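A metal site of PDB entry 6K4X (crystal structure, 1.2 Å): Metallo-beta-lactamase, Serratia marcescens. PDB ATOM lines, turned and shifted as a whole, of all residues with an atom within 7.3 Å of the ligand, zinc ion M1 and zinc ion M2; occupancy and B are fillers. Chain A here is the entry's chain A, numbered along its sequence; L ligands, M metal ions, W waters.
An oxygen (O2) of the ligand is in hydrogen-bond range of the side-chain hydroxyl (OG) of Ser 175 (3.2 Å).
The side-chain hydroxyl of Thr 177 lies within hydrogen-bond range of an oxygen (O2) of the ligand (2.8 Å).
A nitrogen (N1) of the ligand sits at hydrogen-bond distance from the side-chain amide oxygen of Gln 113.
A ring nitrogen (ND1) of His 150 is in hydrogen-bond range of the backbone carbonyl oxygen (O) of Thr 177, 2.9 Å away.
A ring nitrogen (ND1) of His 72 is in hydrogen-bond range of the side-chain carboxylate of Asp 174, 2.7 Å away.
NE2 of His 74 sits at hydrogen-bond distance from OD2 of Asp 111 (2.7 Å).
OD1 of Asp 111 sits at hydrogen-bond distance from N of Gln 113 (2.9 Å).
OG of Ser 116 lies within hydrogen-bond range of O of Gln 113, 2.7 Å away.
Residues that only touch the ligand: Val 179 (3.6 Å).
Hydrophobic or aromatic side chains that line the ligand: His 72, His 150, Val 179 and His 215.
Ten residues have an atom within 4 Å of the ligand: His 72, His 74, Asp 76, His 77, Gln 113, His 150, Ser 175, Thr 177, Val 179 and His 215.
The nearest printed residue that does not touch the ligand is Arg 252 (4.3 Å).
Three residues have an atom within 4 Å of zinc ion M1: Asp 76, His 77 and His 215.
The nearest printed residue that does not touch zinc ion M1 is His 72 (4.2 Å).
Of the 25 residues printed, 3 come within 4 Å of zinc ion M2.
The nearest printed residue that does not touch zinc ion M2 is Gln 113 (4.2 Å).
Zinc ion M1 is bound by a ring nitrogen (NE2) of His 77 (2.0 Å), a ring nitrogen (NE2) of His 215 (2.0 Å), the side-chain carboxylate (OD2) of Asp 76 (2.1 Å), an oxygen (O1) of the ligand (2.3 Å) and a sulfur (S1) of the ligand (2.4 Å).
Zinc ion M2 is bound by a ring nitrogen (NE2) of His 150 (2.0 Å).
NE2 of His 72 binds zinc ion M2, at 2.0 Å.
A ring nitrogen (ND1) of His 74 binds zinc ion M2, at 2.1 Å.
Zinc ion M2 is bound by a sulfur (S1) of the ligand (2.3 Å).
Water W4 lies within hydrogen-bond range of O2 of the ligand (2.8 Å) and OG of Ser 175 (3.5 Å).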
ATOM      1  N   TRP A   5       6.813 -23.151  19.936  1.00  0.00           N
ATOM      2  CA  TRP A   5       5.862 -22.053  19.858  1.00  0.00           C
ATOM      3  C   TRP A   5       5.142 -21.821  21.164  1.00  0.00           C
ATOM      4  O   TRP A   5       4.616 -20.769  21.386  1.00  0.00           O
ATOM      5  CB  TRP A   5       4.774 -22.323  18.816  1.00  0.00           C
ATOM      6  CG  TRP A   5       5.208 -22.334  17.395  1.00  0.00           C
ATOM      7  CD1 TRP A   5       6.395 -21.915  16.887  1.00  0.00           C
ATOM      8  CD2 TRP A   5       4.431 -22.841  16.306  1.00  0.00           C
ATOM      9  NE1 TRP A   5       6.388 -22.086  15.522  1.00  0.00           N
ATOM     10  CE2 TRP A   5       5.212 -22.674  15.148  1.00  0.00           C
ATOM     11  CE3 TRP A   5       3.163 -23.430  16.205  1.00  0.00           C
ATOM     12  CZ2 TRP A   5       4.744 -23.057  13.891  1.00  0.00           C
ATOM     13  CZ3 TRP A   5       2.706 -23.809  14.964  1.00  0.00           C
ATOM     14  CH2 TRP A   5       3.490 -23.635  13.827  1.00  0.00           C
ATOM     15  N   ILE A  26       7.437 -17.710  19.732  1.00  0.00           N
ATOM     16  CA  ILE A  26       6.490 -16.770  19.096  1.00  0.00           C
ATOM     17  C   ILE A  26       6.481 -15.487  19.897  1.00  0.00           C
ATOM     18  O   ILE A  26       6.326 -15.520  21.124  1.00  0.00           O
ATOM     19  CB  ILE A  26       5.065 -17.337  18.986  1.00  0.00           C
ATOM     20  CG1 ILE A  26       5.006 -18.626  18.159  1.00  0.00           C
ATOM     21  CG2 ILE A  26       4.137 -16.284  18.421  1.00  0.00           C
ATOM     22  CD1 ILE A  26       5.245 -18.434  16.687  1.00  0.00           C
ATOM     23  N   HIS A  72      -1.575 -11.576  12.483  1.00  0.00           N
ATOM     24  CA  HIS A  72      -2.380 -12.335  11.573  1.00  0.00           C
ATOM     25  C   HIS A  72      -2.931 -13.582  12.236  1.00  0.00           C
ATOM     26  O   HIS A  72      -2.480 -14.041  13.284  1.00  0.00           O
ATOM     27  CB  HIS A  72      -1.634 -12.664  10.260  1.00  0.00           C
ATOM     28  CG  HIS A  72      -0.599 -13.726  10.370  1.00  0.00           C
ATOM     29  ND1 HIS A  72       0.711 -13.457  10.630  1.00  0.00           N
ATOM     30  CD2 HIS A  72      -0.678 -15.077  10.227  1.00  0.00           C
ATOM     31  CE1 HIS A  72       1.399 -14.583  10.622  1.00  0.00           C
ATOM     32  NE2 HIS A  72       0.565 -15.635  10.396  1.00  0.00           N
ATOM     33  N   SER A  73      -3.947 -14.152  11.562  1.00  0.00           N
ATOM     34  CA  SER A  73      -4.870 -15.133  12.121  1.00  0.00           C
ATOM     35  C   SER A  73      -4.464 -16.564  11.762  1.00  0.00           C
ATOM     36  O   SER A  73      -5.257 -17.286  11.144  1.00  0.00           O
ATOM     37  CB  SER A  73      -6.246 -14.791  11.637  1.00  0.00           C
ATOM     38  OG  SER A  73      -6.263 -14.581  10.226  1.00  0.00           O
ATOM     39  N   HIS A  74      -3.258 -16.965  12.191  1.00  0.00           N
ATOM     40  CA  HIS A  74      -2.867 -18.369  12.195  1.00  0.00           C
ATOM     41  C   HIS A  74      -2.631 -18.793  13.642  1.00  0.00           C
ATOM     42  O   HIS A  74      -2.397 -17.966  14.521  1.00  0.00           O
ATOM     43  CB  HIS A  74      -1.606 -18.632  11.378  1.00  0.00           C
ATOM     44  CG  HIS A  74      -1.811 -18.387   9.915  1.00  0.00           C
ATOM     45  ND1 HIS A  74      -0.807 -18.049   9.069  1.00  0.00           N
ATOM     46  CD2 HIS A  74      -2.927 -18.507   9.177  1.00  0.00           C
ATOM     47  CE1 HIS A  74      -1.315 -17.939   7.859  1.00  0.00           C
ATOM     48  NE2 HIS A  74      -2.606 -18.214   7.897  1.00  0.00           N
ATOM     49  N   GLU A  75      -2.734 -20.098  13.876  1.00  0.00           N
ATOM     50  CA  GLU A  75      -2.762 -20.667  15.218  1.00  0.00           C
ATOM     51  C   GLU A  75      -1.525 -20.311  16.039  1.00  0.00           C
ATOM     52  O   GLU A  75      -1.605 -20.286  17.263  1.00  0.00           O
ATOM     53  CB  GLU A  75      -2.945 -22.179  15.135  1.00  0.00           C
ATOM     54  CG  GLU A  75      -1.724 -22.929  14.622  1.00  0.00           C
ATOM     55  CD  GLU A  75      -1.746 -24.457  14.594  1.00  0.00           C
ATOM     56  OE1 GLU A  75      -2.281 -25.041  15.546  1.00  0.00           O
ATOM     57  OE2 GLU A  75      -1.200 -25.061  13.632  1.00  0.00           O
ATOM     58  N   ASP A  76      -0.370 -20.131  15.412  1.00  0.00           N
ATOM     59  CA  ASP A  76       0.847 -19.856  16.155  1.00  0.00           C
ATOM     60  C   ASP A  76       0.866 -18.444  16.770  1.00  0.00           C
ATOM     61  O   ASP A  76       1.511 -18.259  17.803  1.00  0.00           O
ATOM     62  CB  ASP A  76       2.092 -20.110  15.322  1.00  0.00           C
ATOM     63  CG  ASP A  76       2.210 -19.392  13.993  1.00  0.00           C
ATOM     64  OD1 ASP A  76       1.158 -19.094  13.372  1.00  0.00           O
ATOM     65  OD2 ASP A  76       3.363 -19.174  13.569  1.00  0.00           O
ATOM     66  N   HIS A  77       0.237 -17.466  16.115  1.00  0.00           N
ATOM     67  CA  HIS A  77       0.233 -16.088  16.631  1.00  0.00           C
ATOM     68  C   HIS A  77      -1.057 -15.778  17.383  1.00  0.00           C
ATOM     69  O   HIS A  77      -1.068 -14.917  18.285  1.00  0.00           O
ATOM     70  CB  HIS A  77       0.416 -15.090  15.488  1.00  0.00           C
ATOM     71  CG  HIS A  77       1.597 -15.427  14.657  1.00  0.00           C
ATOM     72  ND1 HIS A  77       2.899 -15.166  15.061  1.00  0.00           N
ATOM     73  CD2 HIS A  77       1.682 -16.110  13.500  1.00  0.00           C
ATOM     74  CE1 HIS A  77       3.712 -15.673  14.140  1.00  0.00           C
ATOM     75  NE2 HIS A  77       3.009 -16.282  13.198  1.00  0.00           N
ATOM     76  N   ASP A 111      -6.653 -18.003   1.824  1.00  0.00           N
ATOM     77  CA  ASP A 111      -5.325 -18.113   2.446  1.00  0.00           C
ATOM     78  C   ASP A 111      -4.490 -19.094   1.623  1.00  0.00           C
ATOM     79  O   ASP A 111      -4.939 -20.209   1.381  1.00  0.00           O
ATOM     80  CB  ASP A 111      -5.483 -18.577   3.889  1.00  0.00           C
ATOM     81  CG  ASP A 111      -4.212 -18.503   4.716  1.00  0.00           C
ATOM     82  OD1 ASP A 111      -3.177 -19.024   4.277  1.00  0.00           O
ATOM     83  OD2 ASP A 111      -4.292 -17.914   5.806  1.00  0.00           O
ATOM     84  N   GLN A 113      -2.238 -21.028   2.477  1.00  0.00           N
ATOM     85  CA  GLN A 113      -2.066 -22.270   3.223  1.00  0.00           C
ATOM     86  C   GLN A 113      -3.366 -23.044   3.412  1.00  0.00           C
ATOM     87  O   GLN A 113      -3.340 -24.123   4.010  1.00  0.00           O
ATOM     88  CB  GLN A 113      -1.414 -21.981   4.574  1.00  0.00           C
ATOM     89  CG  GLN A 113       0.027 -21.553   4.458  1.00  0.00           C
ATOM     90  CD  GLN A 113       0.627 -21.345   5.826  1.00  0.00           C
ATOM     91  OE1 GLN A 113       1.017 -22.302   6.504  1.00  0.00           O
ATOM     92  NE2 GLN A 113       0.646 -20.118   6.312  1.00  0.00           N
ATOM     93  N   SER A 116      -4.049 -26.810   4.704  1.00  0.00           N
ATOM     94  CA  SER A 116      -2.924 -27.276   5.501  1.00  0.00           C
ATOM     95  C   SER A 116      -2.896 -26.597   6.878  1.00  0.00           C
ATOM     96  O   SER A 116      -2.002 -26.864   7.675  1.00  0.00           O
ATOM     97  CB  SER A 116      -1.617 -27.096   4.769  1.00  0.00           C
ATOM     98  OG  SER A 116      -1.254 -25.716   4.710  1.00  0.00           O
ATOM     99  N   LEU A 117      -3.875 -25.744   7.188  1.00  0.00           N
ATOM    100  CA  LEU A 117      -3.856 -24.982   8.439  1.00  0.00           C
ATOM    101  C   LEU A 117      -4.638 -25.728   9.526  1.00  0.00           C
ATOM    102  O   LEU A 117      -5.623 -26.398   9.226  1.00  0.00           O
ATOM    103  CB  LEU A 117      -4.456 -23.596   8.238  1.00  0.00           C
ATOM    104  CG  LEU A 117      -3.648 -22.666   7.349  1.00  0.00           C
ATOM    105  CD1 LEU A 117      -4.502 -21.512   6.833  1.00  0.00           C
ATOM    106  CD2 LEU A 117      -2.421 -22.152   8.090  1.00  0.00           C
ATOM    107  N   HIS A 150       0.609 -12.723   3.327  1.00  0.00           N
ATOM    108  CA  HIS A 150       0.582 -13.973   4.101  1.00  0.00           C
ATOM    109  C   HIS A 150      -0.855 -14.306   4.538  1.00  0.00           C
ATOM    110  O   HIS A 150      -1.239 -15.475   4.561  1.00  0.00           O
ATOM    111  CB  HIS A 150       1.595 -13.898   5.216  1.00  0.00           C
ATOM    112  CG  HIS A 150       1.708 -15.090   6.078  1.00  0.00           C
ATOM    113  ND1 HIS A 150       2.513 -16.145   5.739  1.00  0.00           N
ATOM    114  CD2 HIS A 150       1.186 -15.376   7.285  1.00  0.00           C
ATOM    115  CE1 HIS A 150       2.486 -17.030   6.735  1.00  0.00           C
ATOM    116  NE2 HIS A 150       1.645 -16.615   7.685  1.00  0.00           N
ATOM    117  N   THR A 151      -1.601 -13.255   4.874  1.00  0.00           N
ATOM    118  CA  THR A 151      -3.037 -13.306   5.082  1.00  0.00           C
ATOM    119  C   THR A 151      -3.603 -11.989   4.564  1.00  0.00           C
ATOM    120  O   THR A 151      -2.884 -10.984   4.498  1.00  0.00           O
ATOM    121  CB  THR A 151      -3.458 -13.472   6.562  1.00  0.00           C
ATOM    122  OG1 THR A 151      -3.150 -12.272   7.288  1.00  0.00           O
ATOM    123  CG2 THR A 151      -2.904 -14.704   7.229  1.00  0.00           C
ATOM    124  N   ASP A 174       4.515  -8.046  11.214  1.00  0.00           N
ATOM    125  CA  ASP A 174       3.793  -9.224  10.766  1.00  0.00           C
ATOM    126  C   ASP A 174       4.672 -10.026   9.809  1.00  0.00           C
ATOM    127  O   ASP A 174       5.644  -9.528   9.232  1.00  0.00           O
ATOM    128  CB  ASP A 174       2.501  -8.834  10.066  1.00  0.00           C
ATOM    129  CG  ASP A 174       1.556  -9.991   9.841  1.00  0.00           C
ATOM    130  OD1 ASP A 174       1.708 -10.996  10.533  1.00  0.00           O
ATOM    131  OD2 ASP A 174       0.629  -9.806   9.012  1.00  0.00           O
ATOM    132  N   SER A 175       4.327 -11.312   9.672  1.00  0.00           N
ATOM    133  CA  SER A 175       4.944 -12.208   8.683  1.00  0.00           C
ATOM    134  C   SER A 175       4.645 -11.745   7.269  1.00  0.00           C
ATOM    135  O   SER A 175       3.517 -11.440   6.921  1.00  0.00           O
ATOM    136  CB  SER A 175       4.464 -13.607   8.901  1.00  0.00           C
ATOM    137  OG  SER A 175       4.749 -14.000  10.233  1.00  0.00           O
ATOM    138  N   LEU A 176       5.693 -11.777   6.433  1.00  0.00           N
ATOM    139  CA  LEU A 176       5.609 -11.395   5.026  1.00  0.00           C
ATOM    140  C   LEU A 176       5.939 -12.578   4.116  1.00  0.00           C
ATOM    141  O   LEU A 176       6.434 -12.382   3.000  1.00  0.00           O
ATOM    142  CB  LEU A 176       6.581 -10.252   4.766  1.00  0.00           C
ATOM    143  CG  LEU A 176       6.410  -9.016   5.628  1.00  0.00           C
ATOM    144  CD1 LEU A 176       7.443  -7.967   5.249  1.00  0.00           C
ATOM    145  CD2 LEU A 176       4.991  -8.459   5.543  1.00  0.00           C
ATOM    146  N   THR A 177       5.681 -13.802   4.598  1.00  0.00           N
ATOM    147  CA  THR A 177       6.201 -15.004   3.970  1.00  0.00           C
ATOM    148  C   THR A 177       5.181 -15.616   2.999  1.00  0.00           C
ATOM    149  O   THR A 177       4.030 -15.896   3.326  1.00  0.00           O
ATOM    150  CB  THR A 177       6.552 -16.019   5.059  1.00  0.00           C
ATOM    151  OG1 THR A 177       5.414 -16.176   5.892  1.00  0.00           O
ATOM    152  CG2 THR A 177       7.755 -15.575   5.858  1.00  0.00           C
ATOM    153  N   ALA A 178       5.677 -15.936   1.807  1.00  0.00           N
ATOM    154  CA  ALA A 178       4.958 -16.693   0.787  1.00  0.00           C
ATOM    155  C   ALA A 178       5.136 -18.179   1.093  1.00  0.00           C
ATOM    156  O   ALA A 178       6.238 -18.769   0.934  1.00  0.00           O
ATOM    157  CB  ALA A 178       5.494 -16.357  -0.589  1.00  0.00           C
ATOM    158  N   VAL A 179       4.093 -18.785   1.634  1.00  0.00           N
ATOM    159  CA  VAL A 179       4.072 -20.226   1.991  1.00  0.00           C
ATOM    160  C   VAL A 179       2.671 -20.725   1.651  1.00  0.00           C
ATOM    161  O   VAL A 179       1.714 -19.982   1.699  1.00  0.00           O
ATOM    162  CB  VAL A 179       4.431 -20.418   3.484  1.00  0.00           C
ATOM    163  CG1 VAL A 179       3.564 -19.558   4.371  1.00  0.00           C
ATOM    164  CG2 VAL A 179       4.373 -21.856   3.990  1.00  0.00           C
ATOM    165  N   SER A 180       2.559 -21.985   1.249  1.00  0.00           N
ATOM    166  CA  SER A 180       1.255 -22.448   0.809  1.00  0.00           C
ATOM    167  C   SER A 180       1.092 -23.942   1.005  1.00  0.00           C
ATOM    168  O   SER A 180       2.050 -24.667   1.248  1.00  0.00           O
ATOM    169  CB  SER A 180       1.036 -22.117  -0.640  1.00  0.00           C
ATOM    170  OG  SER A 180       1.780 -22.997  -1.486  1.00  0.00           O
ATOM    171  N   ALA A 214       7.129 -11.267  14.327  1.00  0.00           N
ATOM    172  CA  ALA A 214       6.170 -12.179  14.895  1.00  0.00           C
ATOM    173  C   ALA A 214       6.813 -13.545  15.198  1.00  0.00           C
ATOM    174  O   ALA A 214       6.567 -14.145  16.253  1.00  0.00           O
ATOM    175  CB  ALA A 214       4.975 -12.298  13.976  1.00  0.00           C
ATOM    176  N   HIS A 215       7.621 -14.055  14.269  1.00  0.00           N
ATOM    177  CA  HIS A 215       8.591 -15.106  14.558  1.00  0.00           C
ATOM    178  C   HIS A 215       9.891 -14.441  14.977  1.00  0.00           C
ATOM    179  O   HIS A 215      10.559 -13.814  14.158  1.00  0.00           O
ATOM    180  CB  HIS A 215       8.812 -16.019  13.350  1.00  0.00           C
ATOM    181  CG  HIS A 215       7.634 -16.905  13.085  1.00  0.00           C
ATOM    182  ND1 HIS A 215       7.440 -18.099  13.762  1.00  0.00           N
ATOM    183  CD2 HIS A 215       6.539 -16.739  12.302  1.00  0.00           C
ATOM    184  CE1 HIS A 215       6.286 -18.623  13.395  1.00  0.00           C
ATOM    185  NE2 HIS A 215       5.710 -17.820  12.499  1.00  0.00           N
ATOM    186  N   VAL A 218      13.278 -14.045  13.098  1.00  0.00           N
ATOM    187  CA  VAL A 218      13.350 -13.347  11.856  1.00  0.00           C
ATOM    188  C   VAL A 218      14.259 -12.113  11.976  1.00  0.00           C
ATOM    189  O   VAL A 218      14.959 -11.781  11.019  1.00  0.00           O
ATOM    190  CB  VAL A 218      11.943 -12.995  11.354  1.00  0.00           C
ATOM    191  CG1 VAL A 218      11.949 -11.912  10.289  1.00  0.00           C
ATOM    192  CG2 VAL A 218      11.259 -14.243  10.836  1.00  0.00           C
ATOM    193  N   ARG A 252      11.979 -14.598  -0.620  1.00  0.00           N
ATOM    194  CA  ARG A 252      11.218 -15.829  -0.508  1.00  0.00           C
ATOM    195  C   ARG A 252      10.161 -15.892  -1.621  1.00  0.00           C
ATOM    196  O   ARG A 252       9.964 -16.958  -2.221  1.00  0.00           O
ATOM    197  CB  ARG A 252      10.568 -15.914   0.875  1.00  0.00           C
ATOM    198  CG  ARG A 252       9.820 -17.197   1.139  1.00  0.00           C
ATOM    199  CD  ARG A 252       9.425 -17.312   2.600  1.00  0.00           C
ATOM    200  NE  ARG A 252       8.781 -18.586   2.864  1.00  0.00           N
ATOM    201  CZ  ARG A 252       8.726 -19.200   4.025  1.00  0.00           C
ATOM    202  NH1 ARG A 252       9.300 -18.668   5.086  1.00  0.00           N
ATOM    203  NH2 ARG A 252       8.035 -20.320   4.124  1.00  0.00           N
HETATM  204  O1  LIG L   1       4.277 -16.639  10.197  1.00  0.00           O
HETATM  205  C1  LIG L   1       4.922 -17.168   9.261  1.00  0.00           C
HETATM  206  O2  LIG L   1       5.794 -16.523   8.607  1.00  0.00           O
HETATM  207  C2  LIG L   1       4.680 -18.573   8.859  1.00  0.00           C
HETATM  208  C3  LIG L   1       5.642 -19.140   7.962  1.00  0.00           C
HETATM  209  C4  LIG L   1       3.606 -19.350   9.313  1.00  0.00           C
HETATM  210  S1  LIG L   1       2.398 -18.947  10.456  1.00  0.00           S
HETATM  211  C5  LIG L   1       3.496 -20.672   8.813  1.00  0.00           C
HETATM  212  C6  LIG L   1       4.431 -21.220   7.918  1.00  0.00           C
HETATM  213  N1  LIG L   1       4.312 -22.535   7.484  1.00  0.00           N
HETATM  214  C7  LIG L   1       5.500 -20.458   7.533  1.00  0.00           C
HETATM  215 ZN    ZN M   1       3.712 -17.813  12.052  1.00  0.00          ZN
HETATM  216 ZN    ZN M   2       1.097 -17.355   9.475  1.00  0.00          ZN
HETATM  217  O   HOH W   1       6.161 -24.021   5.589  1.00  0.00           O
HETATM  218  O   HOH W   2       7.694 -19.864  10.557  1.00  0.00           O
HETATM  219  O   HOH W   3       4.855 -21.028  11.699  1.00  0.00           O
HETATM  220  O   HOH W   4       7.969 -14.853   9.187  1.00  0.00           O
